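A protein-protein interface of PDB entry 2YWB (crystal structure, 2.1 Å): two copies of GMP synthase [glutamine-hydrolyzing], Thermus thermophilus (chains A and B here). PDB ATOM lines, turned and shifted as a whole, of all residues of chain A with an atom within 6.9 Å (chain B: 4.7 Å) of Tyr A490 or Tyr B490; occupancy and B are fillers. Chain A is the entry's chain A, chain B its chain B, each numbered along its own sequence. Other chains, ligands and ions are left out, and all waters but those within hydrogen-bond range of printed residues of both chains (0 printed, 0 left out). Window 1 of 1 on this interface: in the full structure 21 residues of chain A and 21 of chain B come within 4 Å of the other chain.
O of Val A488 sits at hydrogen-bond distance from N of Leu B492, at 2.9 Å.
The backbone carbonyl oxygen of Tyr B490 is in hydrogen-bond range of the backbone NH of Tyr A490, at 2.9 Å.
N of Leu A492 sits at hydrogen-bond distance from O of Val B488 (2.8 Å).
OG1 of Thr A493 sits at hydrogen-bond distance from N of Val B488.
O of Val A488 sits close to OD2 of Asp B491.
OD1 of Asp A491 sits close to O of Val B488 (3.4 Å).
The backbone NH (N) of Val A489 lies within hydrogen-bond range of the backbone carbonyl oxygen (O) of Leu A448, at 2.8 Å.
The backbone carbonyl oxygen of Leu A450 is in hydrogen-bond range of the backbone NH of Asp A491, at 3.0 Å.
The guanidinium group (NH1) of Arg A451 lies within salt-bridge range of the side-chain carboxylate (OD2) of Asp A491, at 3.6 Å.
N of Leu B450 lies within hydrogen-bond range of O of Val B489, at 2.7 Å.
The backbone NH (N) of Asp B491 lies within hydrogen-bond range of the backbone carbonyl oxygen (O) of Leu B450 (2.9 Å).
The side-chain hydroxyl (OH) of Tyr B490 is in hydrogen-bond range of the backbone carbonyl oxygen (O) of Ala B452 (3.5 Å).
Among the printed residues, pairs that only touch across the chains: Val A489 with Tyr B490 (3.2 Å), Tyr A490 with Val B489 (3.2 Å), Leu A468 with Leu B466 (3.5 Å), Leu A468 with Trp B463 (3.6 Å), Tyr A490 with Leu B492 (3.7 Å), Leu A492 with Tyr B490 (3.7 Å), Leu A492 with Leu B471 (3.9 Å), Val A489 with Val B489 (3.9 Å), Trp A502 with Val B489 (3.9 Å), Asp A491 with Val B489 (3.9 Å), Val A489 with Leu B492 (3.9 Å) and Val A489 with Asp B491 (3.97 Å).
Of chain B, only Val B489, Tyr B490 and Leu B492 come within 4 Å of Tyr A490.
Printed residues of chain A within 4 Å of Tyr B490: Val A489 (3.2 Å), Tyr A490 (2.9 Å) and Leu A492 (3.7 Å).
Of the printed residues of chain A, Asp B491 touches Val A488 and Val A489.
Printed residues of chain B within 4 Å of Thr A493: Val B488 (3.0 Å).
Of the printed residues of chain B, Val A488 touches Asp B491 and Leu B492.
Printed residues of chain A within 4 Å of Val B488: Asp A491 (3.4 Å), Leu A492 (2.8 Å) and Thr A493 (3.0 Å).
The nearest printed residue of chain B that does not touch Val A489 is Leu B450 (6.3 Å).
Hydrophobic or aromatic side chains of chain B within 4 Å of the printed part of chain A: Trp B463, Leu B471, Val B489, Tyr B490 and Leu B492.
Printed residues of chain A that touch a printed residue of chain B: Leu A468, Val A488, Val A489, Tyr A490, Asp A491, Leu A492, Thr A493 and Trp A502.
Among the printed residues, no Asp or Glu carboxylate lies within 4 Å of a Lys or Arg side-chain nitrogen of the other chain.
Val A488 touches Leu B492, and with the chains exchanged Leu A492 touches Val B488.
Val A489 touches its own counterpart, Val B489.
Val A489 touches Tyr B490, and with the chains exchanged Tyr A490 touches Val B489.
Leu A492 touches Leu B471, but with the chains exchanged Leu A471 does not touch Leu B492 (4.04 Å).
Of the 18 pairs that touch across the chains among the printed residues, 12 have their exchanged pair printed and touching as well.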
ATOM      1  N   PHE A 409      41.719  16.444 -23.478  1.00  0.00           N
ATOM      2  CA  PHE A 409      40.324  16.701 -23.838  1.00  0.00           C
ATOM      3  C   PHE A 409      40.244  17.917 -24.766  1.00  0.00           C
ATOM      4  O   PHE A 409      39.671  17.848 -25.858  1.00  0.00           O
ATOM      5  CB  PHE A 409      39.516  16.943 -22.552  1.00  0.00           C
ATOM      6  CG  PHE A 409      38.043  17.209 -22.771  1.00  0.00           C
ATOM      7  CD1 PHE A 409      37.316  16.498 -23.719  1.00  0.00           C
ATOM      8  CD2 PHE A 409      37.368  18.122 -21.960  1.00  0.00           C
ATOM      9  CE1 PHE A 409      35.944  16.685 -23.854  1.00  0.00           C
ATOM     10  CE2 PHE A 409      35.999  18.316 -22.086  1.00  0.00           C
ATOM     11  CZ  PHE A 409      35.283  17.597 -23.034  1.00  0.00           C
ATOM     12  N   VAL A 422      31.074  24.365 -28.820  1.00  0.00           N
ATOM     13  CA  VAL A 422      30.517  24.242 -27.480  1.00  0.00           C
ATOM     14  C   VAL A 422      30.886  25.566 -26.804  1.00  0.00           C
ATOM     15  O   VAL A 422      31.865  26.216 -27.189  1.00  0.00           O
ATOM     16  CB  VAL A 422      31.097  23.044 -26.644  1.00  0.00           C
ATOM     17  CG1 VAL A 422      30.699  21.714 -27.295  1.00  0.00           C
ATOM     18  CG2 VAL A 422      32.630  23.174 -26.476  1.00  0.00           C
ATOM     19  N   LEU A 448      37.484  10.610 -13.999  1.00  0.00           N
ATOM     20  CA  LEU A 448      37.502  11.917 -14.624  1.00  0.00           C
ATOM     21  C   LEU A 448      36.188  12.178 -15.341  1.00  0.00           C
ATOM     22  O   LEU A 448      35.709  11.346 -16.115  1.00  0.00           O
ATOM     23  CB  LEU A 448      38.658  12.038 -15.621  1.00  0.00           C
ATOM     24  CG  LEU A 448      38.802  13.485 -16.123  1.00  0.00           C
ATOM     25  CD1 LEU A 448      39.869  14.213 -15.320  1.00  0.00           C
ATOM     26  CD2 LEU A 448      39.146  13.490 -17.587  1.00  0.00           C
ATOM     27  N   ALA A 449      35.599  13.336 -15.079  1.00  0.00           N
ATOM     28  CA  ALA A 449      34.346  13.680 -15.724  1.00  0.00           C
ATOM     29  C   ALA A 449      34.561  14.736 -16.790  1.00  0.00           C
ATOM     30  O   ALA A 449      35.153  15.791 -16.522  1.00  0.00           O
ATOM     31  CB  ALA A 449      33.332  14.177 -14.682  1.00  0.00           C
ATOM     32  N   LEU A 450      34.107  14.439 -18.009  1.00  0.00           N
ATOM     33  CA  LEU A 450      34.196  15.395 -19.108  1.00  0.00           C
ATOM     34  C   LEU A 450      32.887  16.195 -19.055  1.00  0.00           C
ATOM     35  O   LEU A 450      31.807  15.629 -18.922  1.00  0.00           O
ATOM     36  CB  LEU A 450      34.351  14.660 -20.451  1.00  0.00           C
ATOM     37  CG  LEU A 450      35.590  13.753 -20.537  1.00  0.00           C
ATOM     38  CD1 LEU A 450      35.585  12.977 -21.859  1.00  0.00           C
ATOM     39  CD2 LEU A 450      36.864  14.617 -20.403  1.00  0.00           C
ATOM     40  N   ARG A 451      32.983  17.511 -19.177  1.00  0.00           N
ATOM     41  CA  ARG A 451      31.813  18.364 -19.085  1.00  0.00           C
ATOM     42  C   ARG A 451      31.796  19.400 -20.200  1.00  0.00           C
ATOM     43  O   ARG A 451      32.654  20.270 -20.238  1.00  0.00           O
ATOM     44  CB  ARG A 451      31.838  19.086 -17.730  1.00  0.00           C
ATOM     45  CG  ARG A 451      30.479  19.404 -17.099  1.00  0.00           C
ATOM     46  CD  ARG A 451      29.788  20.590 -17.720  1.00  0.00           C
ATOM     47  NE  ARG A 451      28.630  21.012 -16.925  1.00  0.00           N
ATOM     48  CZ  ARG A 451      27.408  20.509 -17.026  1.00  0.00           C
ATOM     49  NH1 ARG A 451      27.140  19.549 -17.904  1.00  0.00           N
ATOM     50  NH2 ARG A 451      26.454  20.960 -16.224  1.00  0.00           N
ATOM     51  N   ALA A 452      30.831  19.311 -21.110  1.00  0.00           N
ATOM     52  CA  ALA A 452      30.726  20.310 -22.167  1.00  0.00           C
ATOM     53  C   ALA A 452      29.269  20.771 -22.283  1.00  0.00           C
ATOM     54  O   ALA A 452      28.337  19.983 -22.097  1.00  0.00           O
ATOM     55  CB  ALA A 452      31.213  19.755 -23.489  1.00  0.00           C
ATOM     56  N   VAL A 453      29.067  22.051 -22.566  1.00  0.00           N
ATOM     57  CA  VAL A 453      27.704  22.551 -22.694  1.00  0.00           C
ATOM     58  C   VAL A 453      27.583  23.474 -23.885  1.00  0.00           C
ATOM     59  O   VAL A 453      28.583  23.954 -24.410  1.00  0.00           O
ATOM     60  CB  VAL A 453      27.254  23.330 -21.429  1.00  0.00           C
ATOM     61  CG1 VAL A 453      27.241  22.408 -20.204  1.00  0.00           C
ATOM     62  CG2 VAL A 453      28.186  24.522 -21.200  1.00  0.00           C
ATOM     63  N   ASP A 462      22.776  23.491 -21.989  1.00  0.00           N
ATOM     64  CA  ASP A 462      22.469  22.069 -22.110  1.00  0.00           C
ATOM     65  C   ASP A 462      23.756  21.269 -22.191  1.00  0.00           C
ATOM     66  O   ASP A 462      24.736  21.751 -22.743  1.00  0.00           O
ATOM     67  CB  ASP A 462      21.649  21.804 -23.372  1.00  0.00           C
ATOM     68  CG  ASP A 462      20.356  22.581 -23.397  1.00  0.00           C
ATOM     69  OD1 ASP A 462      19.659  22.600 -22.363  1.00  0.00           O
ATOM     70  OD2 ASP A 462      20.038  23.164 -24.455  1.00  0.00           O
ATOM     71  N   TRP A 463      23.770  20.056 -21.649  1.00  0.00           N
ATOM     72  CA  TRP A 463      24.982  19.253 -21.770  1.00  0.00           C
ATOM     73  C   TRP A 463      25.135  19.066 -23.283  1.00  0.00           C
ATOM     74  O   TRP A 463      24.153  18.794 -23.971  1.00  0.00           O
ATOM     75  CB  TRP A 463      24.846  17.906 -21.049  1.00  0.00           C
ATOM     76  CG  TRP A 463      23.737  17.009 -21.506  1.00  0.00           C
ATOM     77  CD1 TRP A 463      22.433  17.054 -21.113  1.00  0.00           C
ATOM     78  CD2 TRP A 463      23.859  15.857 -22.351  1.00  0.00           C
ATOM     79  NE1 TRP A 463      21.737  15.996 -21.644  1.00  0.00           N
ATOM     80  CE2 TRP A 463      22.586  15.244 -22.407  1.00  0.00           C
ATOM     81  CE3 TRP A 463      24.921  15.281 -23.061  1.00  0.00           C
ATOM     82  CZ2 TRP A 463      22.346  14.075 -23.147  1.00  0.00           C
ATOM     83  CZ3 TRP A 463      24.683  14.119 -23.798  1.00  0.00           C
ATOM     84  CH2 TRP A 463      23.403  13.528 -23.831  1.00  0.00           C
ATOM     85  N   ALA A 464      26.351  19.250 -23.797  1.00  0.00           N
ATOM     86  CA  ALA A 464      26.598  19.155 -25.231  1.00  0.00           C
ATOM     87  C   ALA A 464      26.371  17.778 -25.864  1.00  0.00           C
ATOM     88  O   ALA A 464      26.910  16.769 -25.411  1.00  0.00           O
ATOM     89  CB  ALA A 464      28.022  19.652 -25.550  1.00  0.00           C
ATOM     90  N   ARG A 465      25.580  17.762 -26.933  1.00  0.00           N
ATOM     91  CA  ARG A 465      25.294  16.528 -27.657  1.00  0.00           C
ATOM     92  C   ARG A 465      26.468  16.317 -28.599  1.00  0.00           C
ATOM     93  O   ARG A 465      26.379  16.605 -29.781  1.00  0.00           O
ATOM     94  CB  ARG A 465      24.001  16.660 -28.479  1.00  0.00           C
ATOM     95  CG  ARG A 465      22.758  17.028 -27.666  1.00  0.00           C
ATOM     96  CD  ARG A 465      22.494  16.031 -26.542  1.00  0.00           C
ATOM     97  NE  ARG A 465      21.467  16.503 -25.615  1.00  0.00           N
ATOM     98  CZ  ARG A 465      20.165  16.250 -25.723  1.00  0.00           C
ATOM     99  NH1 ARG A 465      19.690  15.507 -26.730  1.00  0.00           N
ATOM    100  NH2 ARG A 465      19.330  16.748 -24.814  1.00  0.00           N
ATOM    101  N   LEU A 466      27.579  15.847 -28.056  1.00  0.00           N
ATOM    102  CA  LEU A 466      28.775  15.612 -28.848  1.00  0.00           C
ATOM    103  C   LEU A 466      28.729  14.238 -29.522  1.00  0.00           C
ATOM    104  O   LEU A 466      28.071  13.325 -29.041  1.00  0.00           O
ATOM    105  CB  LEU A 466      30.016  15.693 -27.943  1.00  0.00           C
ATOM    106  CG  LEU A 466      30.385  17.093 -27.440  1.00  0.00           C
ATOM    107  CD1 LEU A 466      31.477  17.002 -26.403  1.00  0.00           C
ATOM    108  CD2 LEU A 466      30.818  17.963 -28.633  1.00  0.00           C
ATOM    109  N   LEU A 468      29.285  10.576 -30.263  1.00  0.00           N
ATOM    110  CA  LEU A 468      29.739   9.530 -29.350  1.00  0.00           C
ATOM    111  C   LEU A 468      31.126   8.980 -29.715  1.00  0.00           C
ATOM    112  O   LEU A 468      31.883   8.549 -28.840  1.00  0.00           O
ATOM    113  CB  LEU A 468      28.713   8.386 -29.284  1.00  0.00           C
ATOM    114  CG  LEU A 468      27.365   8.742 -28.625  1.00  0.00           C
ATOM    115  CD1 LEU A 468      26.471   7.517 -28.550  1.00  0.00           C
ATOM    116  CD2 LEU A 468      27.612   9.286 -27.215  1.00  0.00           C
ATOM    117  N   LEU A 471      33.603  11.123 -27.935  1.00  0.00           N
ATOM    118  CA  LEU A 471      33.637  10.807 -26.507  1.00  0.00           C
ATOM    119  C   LEU A 471      34.403   9.504 -26.273  1.00  0.00           C
ATOM    120  O   LEU A 471      35.089   9.342 -25.261  1.00  0.00           O
ATOM    121  CB  LEU A 471      32.216  10.655 -25.957  1.00  0.00           C
ATOM    122  CG  LEU A 471      31.320  11.899 -25.966  1.00  0.00           C
ATOM    123  CD1 LEU A 471      29.970  11.553 -25.334  1.00  0.00           C
ATOM    124  CD2 LEU A 471      31.994  13.023 -25.189  1.00  0.00           C
ATOM    125  N   VAL A 488      36.482   7.238 -17.126  1.00  0.00           N
ATOM    126  CA  VAL A 488      36.089   8.527 -17.674  1.00  0.00           C
ATOM    127  C   VAL A 488      34.581   8.512 -17.848  1.00  0.00           C
ATOM    128  O   VAL A 488      34.020   7.511 -18.311  1.00  0.00           O
ATOM    129  CB  VAL A 488      36.752   8.780 -19.050  1.00  0.00           C
ATOM    130  CG1 VAL A 488      36.286  10.109 -19.628  1.00  0.00           C
ATOM    131  CG2 VAL A 488      38.266   8.750 -18.910  1.00  0.00           C
ATOM    132  N   VAL A 489      33.921   9.608 -17.464  1.00  0.00           N
ATOM    133  CA  VAL A 489      32.467   9.706 -17.591  1.00  0.00           C
ATOM    134  C   VAL A 489      32.129  11.020 -18.278  1.00  0.00           C
ATOM    135  O   VAL A 489      32.982  11.897 -18.391  1.00  0.00           O
ATOM    136  CB  VAL A 489      31.763   9.669 -16.205  1.00  0.00           C
ATOM    137  CG1 VAL A 489      32.138   8.402 -15.452  1.00  0.00           C
ATOM    138  CG2 VAL A 489      32.170  10.888 -15.377  1.00  0.00           C
ATOM    139  N   TYR A 490      30.887  11.151 -18.739  1.00  0.00           N
ATOM    140  CA  TYR A 490      30.447  12.368 -19.405  1.00  0.00           C
ATOM    141  C   TYR A 490      29.244  12.888 -18.642  1.00  0.00           C
ATOM    142  O   TYR A 490      28.304  12.143 -18.357  1.00  0.00           O
ATOM    143  CB  TYR A 490      30.069  12.088 -20.875  1.00  0.00           C
ATOM    144  CG  TYR A 490      29.781  13.352 -21.672  1.00  0.00           C
ATOM    145  CD1 TYR A 490      30.633  14.443 -21.588  1.00  0.00           C
ATOM    146  CD2 TYR A 490      28.644  13.465 -22.482  1.00  0.00           C
ATOM    147  CE1 TYR A 490      30.377  15.623 -22.272  1.00  0.00           C
ATOM    148  CE2 TYR A 490      28.376  14.652 -23.184  1.00  0.00           C
ATOM    149  CZ  TYR A 490      29.256  15.731 -23.071  1.00  0.00           C
ATOM    150  OH  TYR A 490      29.055  16.910 -23.772  1.00  0.00           O
ATOM    151  N   ASP A 491      29.269  14.172 -18.316  1.00  0.00           N
ATOM    152  CA  ASP A 491      28.183  14.791 -17.560  1.00  0.00           C
ATOM    153  C   ASP A 491      26.947  14.954 -18.445  1.00  0.00           C
ATOM    154  O   ASP A 491      27.025  15.555 -19.521  1.00  0.00           O
ATOM    155  CB  ASP A 491      28.631  16.162 -17.072  1.00  0.00           C
ATOM    156  CG  ASP A 491      27.784  16.691 -15.937  1.00  0.00           C
ATOM    157  OD1 ASP A 491      26.591  16.339 -15.830  1.00  0.00           O
ATOM    158  OD2 ASP A 491      28.328  17.489 -15.160  1.00  0.00           O
ATOM    159  N   LEU A 492      25.813  14.439 -17.978  1.00  0.00           N
ATOM    160  CA  LEU A 492      24.550  14.524 -18.714  1.00  0.00           C
ATOM    161  C   LEU A 492      23.601  15.535 -18.061  1.00  0.00           C
ATOM    162  O   LEU A 492      22.392  15.500 -18.301  1.00  0.00           O
ATOM    163  CB  LEU A 492      23.860  13.153 -18.721  1.00  0.00           C
ATOM    164  CG  LEU A 492      24.623  11.962 -19.319  1.00  0.00           C
ATOM    165  CD1 LEU A 492      23.861  10.676 -19.020  1.00  0.00           C
ATOM    166  CD2 LEU A 492      24.786  12.146 -20.820  1.00  0.00           C
ATOM    167  N   THR A 493      24.142  16.441 -17.254  1.00  0.00           N
ATOM    168  CA  THR A 493      23.295  17.392 -16.541  1.00  0.00           C
ATOM    169  C   THR A 493      23.280  18.804 -17.104  1.00  0.00           C
ATOM    170  O   THR A 493      24.322  19.409 -17.328  1.00  0.00           O
ATOM    171  CB  THR A 493      23.701  17.446 -15.046  1.00  0.00           C
ATOM    172  OG1 THR A 493      23.979  16.117 -14.583  1.00  0.00           O
ATOM    173  CG2 THR A 493      22.565  18.037 -14.201  1.00  0.00           C
ATOM    174  N   TRP A 502      31.538  22.131 -11.485  1.00  0.00           N
ATOM    175  CA  TRP A 502      31.054  21.208 -10.460  1.00  0.00           C
ATOM    176  C   TRP A 502      31.102  21.746  -9.024  1.00  0.00           C
ATOM    177  O   TRP A 502      30.492  21.170  -8.125  1.00  0.00           O
ATOM    178  CB  TRP A 502      31.820  19.885 -10.552  1.00  0.00           C
ATOM    179  CG  TRP A 502      31.280  18.971 -11.628  1.00  0.00           C
ATOM    180  CD1 TRP A 502      30.809  19.342 -12.862  1.00  0.00           C
ATOM    181  CD2 TRP A 502      31.165  17.544 -11.569  1.00  0.00           C
ATOM    182  NE1 TRP A 502      30.407  18.236 -13.569  1.00  0.00           N
ATOM    183  CE2 TRP A 502      30.616  17.118 -12.802  1.00  0.00           C
ATOM    184  CE3 TRP A 502      31.471  16.586 -10.601  1.00  0.00           C
ATOM    185  CZ2 TRP A 502      30.367  15.762 -13.088  1.00  0.00           C
ATOM    186  CZ3 TRP A 502      31.223  15.236 -10.885  1.00  0.00           C
ATOM    187  CH2 TRP A 502      30.676  14.841 -12.117  1.00  0.00           C
ATOM    188  N   LEU B 450      25.559   6.447 -14.665  1.00  0.00           N
ATOM    189  CA  LEU B 450      24.801   5.432 -15.388  1.00  0.00           C
ATOM    190  C   LEU B 450      25.878   4.613 -16.126  1.00  0.00           C
ATOM    191  O   LEU B 450      26.850   5.174 -16.663  1.00  0.00           O
ATOM    192  CB  LEU B 450      23.819   6.085 -16.363  1.00  0.00           C
ATOM    193  CG  LEU B 450      22.670   6.912 -15.742  1.00  0.00           C
ATOM    194  CD1 LEU B 450      21.842   7.575 -16.837  1.00  0.00           C
ATOM    195  CD2 LEU B 450      21.774   6.003 -14.898  1.00  0.00           C
ATOM    196  N   ARG B 451      25.712   3.296 -16.148  1.00  0.00           N
ATOM    197  CA  ARG B 451      26.695   2.413 -16.754  1.00  0.00           C
ATOM    198  C   ARG B 451      26.061   1.267 -17.546  1.00  0.00           C
ATOM    199  O   ARG B 451      25.387   0.412 -16.976  1.00  0.00           O
ATOM    200  CB  ARG B 451      27.585   1.865 -15.629  1.00  0.00           C
ATOM    201  CG  ARG B 451      28.395   0.629 -15.942  1.00  0.00           C
ATOM    202  CD  ARG B 451      29.383   0.885 -17.069  1.00  0.00           C
ATOM    203  NE  ARG B 451      30.582   0.064 -16.999  1.00  0.00           N
ATOM    204  CZ  ARG B 451      31.559   0.174 -17.884  1.00  0.00           C
ATOM    205  NH1 ARG B 451      31.430   1.051 -18.869  1.00  0.00           N
ATOM    206  NH2 ARG B 451      32.662  -0.547 -17.770  1.00  0.00           N
ATOM    207  N   ALA B 452      26.267   1.258 -18.861  1.00  0.00           N
ATOM    208  CA  ALA B 452      25.715   0.190 -19.689  1.00  0.00           C
ATOM    209  C   ALA B 452      26.754  -0.290 -20.718  1.00  0.00           C
ATOM    210  O   ALA B 452      27.547   0.493 -21.234  1.00  0.00           O
ATOM    211  CB  ALA B 452      24.456   0.666 -20.385  1.00  0.00           C
ATOM    212  N   TRP B 463      31.326   0.363 -23.800  1.00  0.00           N
ATOM    213  CA  TRP B 463      30.287   1.157 -23.170  1.00  0.00           C
ATOM    214  C   TRP B 463      29.205   1.218 -24.239  1.00  0.00           C
ATOM    215  O   TRP B 463      29.506   1.391 -25.424  1.00  0.00           O
ATOM    216  CB  TRP B 463      30.780   2.565 -22.793  1.00  0.00           C
ATOM    217  CG  TRP B 463      31.362   3.426 -23.885  1.00  0.00           C
ATOM    218  CD1 TRP B 463      32.647   3.399 -24.365  1.00  0.00           C
ATOM    219  CD2 TRP B 463      30.710   4.512 -24.555  1.00  0.00           C
ATOM    220  NE1 TRP B 463      32.832   4.404 -25.283  1.00  0.00           N
ATOM    221  CE2 TRP B 463      31.663   5.105 -25.418  1.00  0.00           C
ATOM    222  CE3 TRP B 463      29.415   5.047 -24.509  1.00  0.00           C
ATOM    223  CZ2 TRP B 463      31.363   6.206 -26.224  1.00  0.00           C
ATOM    224  CZ3 TRP B 463      29.115   6.148 -25.320  1.00  0.00           C
ATOM    225  CH2 TRP B 463      30.090   6.711 -26.164  1.00  0.00           C
ATOM    226  N   ALA B 464      27.950   1.046 -23.841  1.00  0.00           N
ATOM    227  CA  ALA B 464      26.855   1.055 -24.810  1.00  0.00           C
ATOM    228  C   ALA B 464      26.672   2.413 -25.481  1.00  0.00           C
ATOM    229  O   ALA B 464      26.650   3.443 -24.809  1.00  0.00           O
ATOM    230  CB  ALA B 464      25.533   0.614 -24.131  1.00  0.00           C
ATOM    231  N   LEU B 466      24.323   4.316 -26.469  1.00  0.00           N
ATOM    232  CA  LEU B 466      22.894   4.563 -26.359  1.00  0.00           C
ATOM    233  C   LEU B 466      22.509   5.885 -26.993  1.00  0.00           C
ATOM    234  O   LEU B 466      23.355   6.740 -27.240  1.00  0.00           O
ATOM    235  CB  LEU B 466      22.472   4.547 -24.887  1.00  0.00           C
ATOM    236  CG  LEU B 466      22.576   3.216 -24.137  1.00  0.00           C
ATOM    237  CD1 LEU B 466      22.491   3.454 -22.636  1.00  0.00           C
ATOM    238  CD2 LEU B 466      21.477   2.276 -24.616  1.00  0.00           C
ATOM    239  N   LEU B 471      19.592   9.176 -22.912  1.00  0.00           N
ATOM    240  CA  LEU B 471      20.416   9.511 -21.757  1.00  0.00           C
ATOM    241  C   LEU B 471      19.909  10.798 -21.122  1.00  0.00           C
ATOM    242  O   LEU B 471      19.885  10.921 -19.895  1.00  0.00           O
ATOM    243  CB  LEU B 471      21.875   9.664 -22.173  1.00  0.00           C
ATOM    244  CG  LEU B 471      22.532   8.355 -22.635  1.00  0.00           C
ATOM    245  CD1 LEU B 471      23.976   8.617 -23.044  1.00  0.00           C
ATOM    246  CD2 LEU B 471      22.457   7.313 -21.516  1.00  0.00           C
ATOM    247  N   VAL B 488      24.022  13.644 -12.890  1.00  0.00           N
ATOM    248  CA  VAL B 488      24.025  12.344 -13.547  1.00  0.00           C
ATOM    249  C   VAL B 488      25.048  12.334 -14.682  1.00  0.00           C
ATOM    250  O   VAL B 488      25.095  13.257 -15.505  1.00  0.00           O
ATOM    251  CB  VAL B 488      22.629  11.996 -14.109  1.00  0.00           C
ATOM    252  CG1 VAL B 488      22.671  10.608 -14.775  1.00  0.00           C
ATOM    253  CG2 VAL B 488      21.591  11.996 -12.967  1.00  0.00           C
ATOM    254  N   VAL B 489      25.867  11.285 -14.696  1.00  0.00           N
ATOM    255  CA  VAL B 489      26.923  11.099 -15.687  1.00  0.00           C
ATOM    256  C   VAL B 489      26.804   9.712 -16.326  1.00  0.00           C
ATOM    257  O   VAL B 489      26.144   8.819 -15.779  1.00  0.00           O
ATOM    258  CB  VAL B 489      28.323  11.185 -15.034  1.00  0.00           C
ATOM    259  CG1 VAL B 489      28.508  12.532 -14.348  1.00  0.00           C
ATOM    260  CG2 VAL B 489      28.486  10.048 -14.012  1.00  0.00           C
ATOM    261  N   TYR B 490      27.443   9.543 -17.483  1.00  0.00           N
ATOM    262  CA  TYR B 490      27.428   8.264 -18.187  1.00  0.00           C
ATOM    263  C   TYR B 490      28.872   7.774 -18.307  1.00  0.00           C
ATOM    264  O   TYR B 490      29.756   8.535 -18.689  1.00  0.00           O
ATOM    265  CB  TYR B 490      26.799   8.423 -19.579  1.00  0.00           C
ATOM    266  CG  TYR B 490      26.560   7.107 -20.295  1.00  0.00           C
ATOM    267  CD1 TYR B 490      25.831   6.089 -19.684  1.00  0.00           C
ATOM    268  CD2 TYR B 490      27.074   6.873 -21.575  1.00  0.00           C
ATOM    269  CE1 TYR B 490      25.621   4.870 -20.313  1.00  0.00           C
ATOM    270  CE2 TYR B 490      26.870   5.649 -22.224  1.00  0.00           C
ATOM    271  CZ  TYR B 490      26.141   4.650 -21.580  1.00  0.00           C
ATOM    272  OH  TYR B 490      25.927   3.427 -22.180  1.00  0.00           O
ATOM    273  N   ASP B 491      29.099   6.511 -17.968  1.00  0.00           N
ATOM    274  CA  ASP B 491      30.430   5.905 -18.016  1.00  0.00           C
ATOM    275  C   ASP B 491      30.854   5.631 -19.463  1.00  0.00           C
ATOM    276  O   ASP B 491      30.158   4.930 -20.197  1.00  0.00           O
ATOM    277  CB  ASP B 491      30.418   4.608 -17.197  1.00  0.00           C
ATOM    278  CG  ASP B 491      31.809   4.015 -16.990  1.00  0.00           C
ATOM    279  OD1 ASP B 491      31.957   3.195 -16.048  1.00  0.00           O
ATOM    280  OD2 ASP B 491      32.739   4.360 -17.756  1.00  0.00           O
ATOM    281  N   LEU B 492      31.997   6.184 -19.863  1.00  0.00           N
ATOM    282  CA  LEU B 492      32.505   6.016 -21.225  1.00  0.00           C
ATOM    283  C   LEU B 492      33.681   5.057 -21.255  1.00  0.00           C
ATOM    284  O   LEU B 492      34.459   5.064 -22.203  1.00  0.00           O
ATOM    285  CB  LEU B 492      32.972   7.360 -21.795  1.00  0.00           C
ATOM    286  CG  LEU B 492      32.006   8.548 -21.774  1.00  0.00           C
ATOM    287  CD1 LEU B 492      32.783   9.849 -21.988  1.00  0.00           C
ATOM    288  CD2 LEU B 492      30.945   8.362 -22.834  1.00  0.00           C
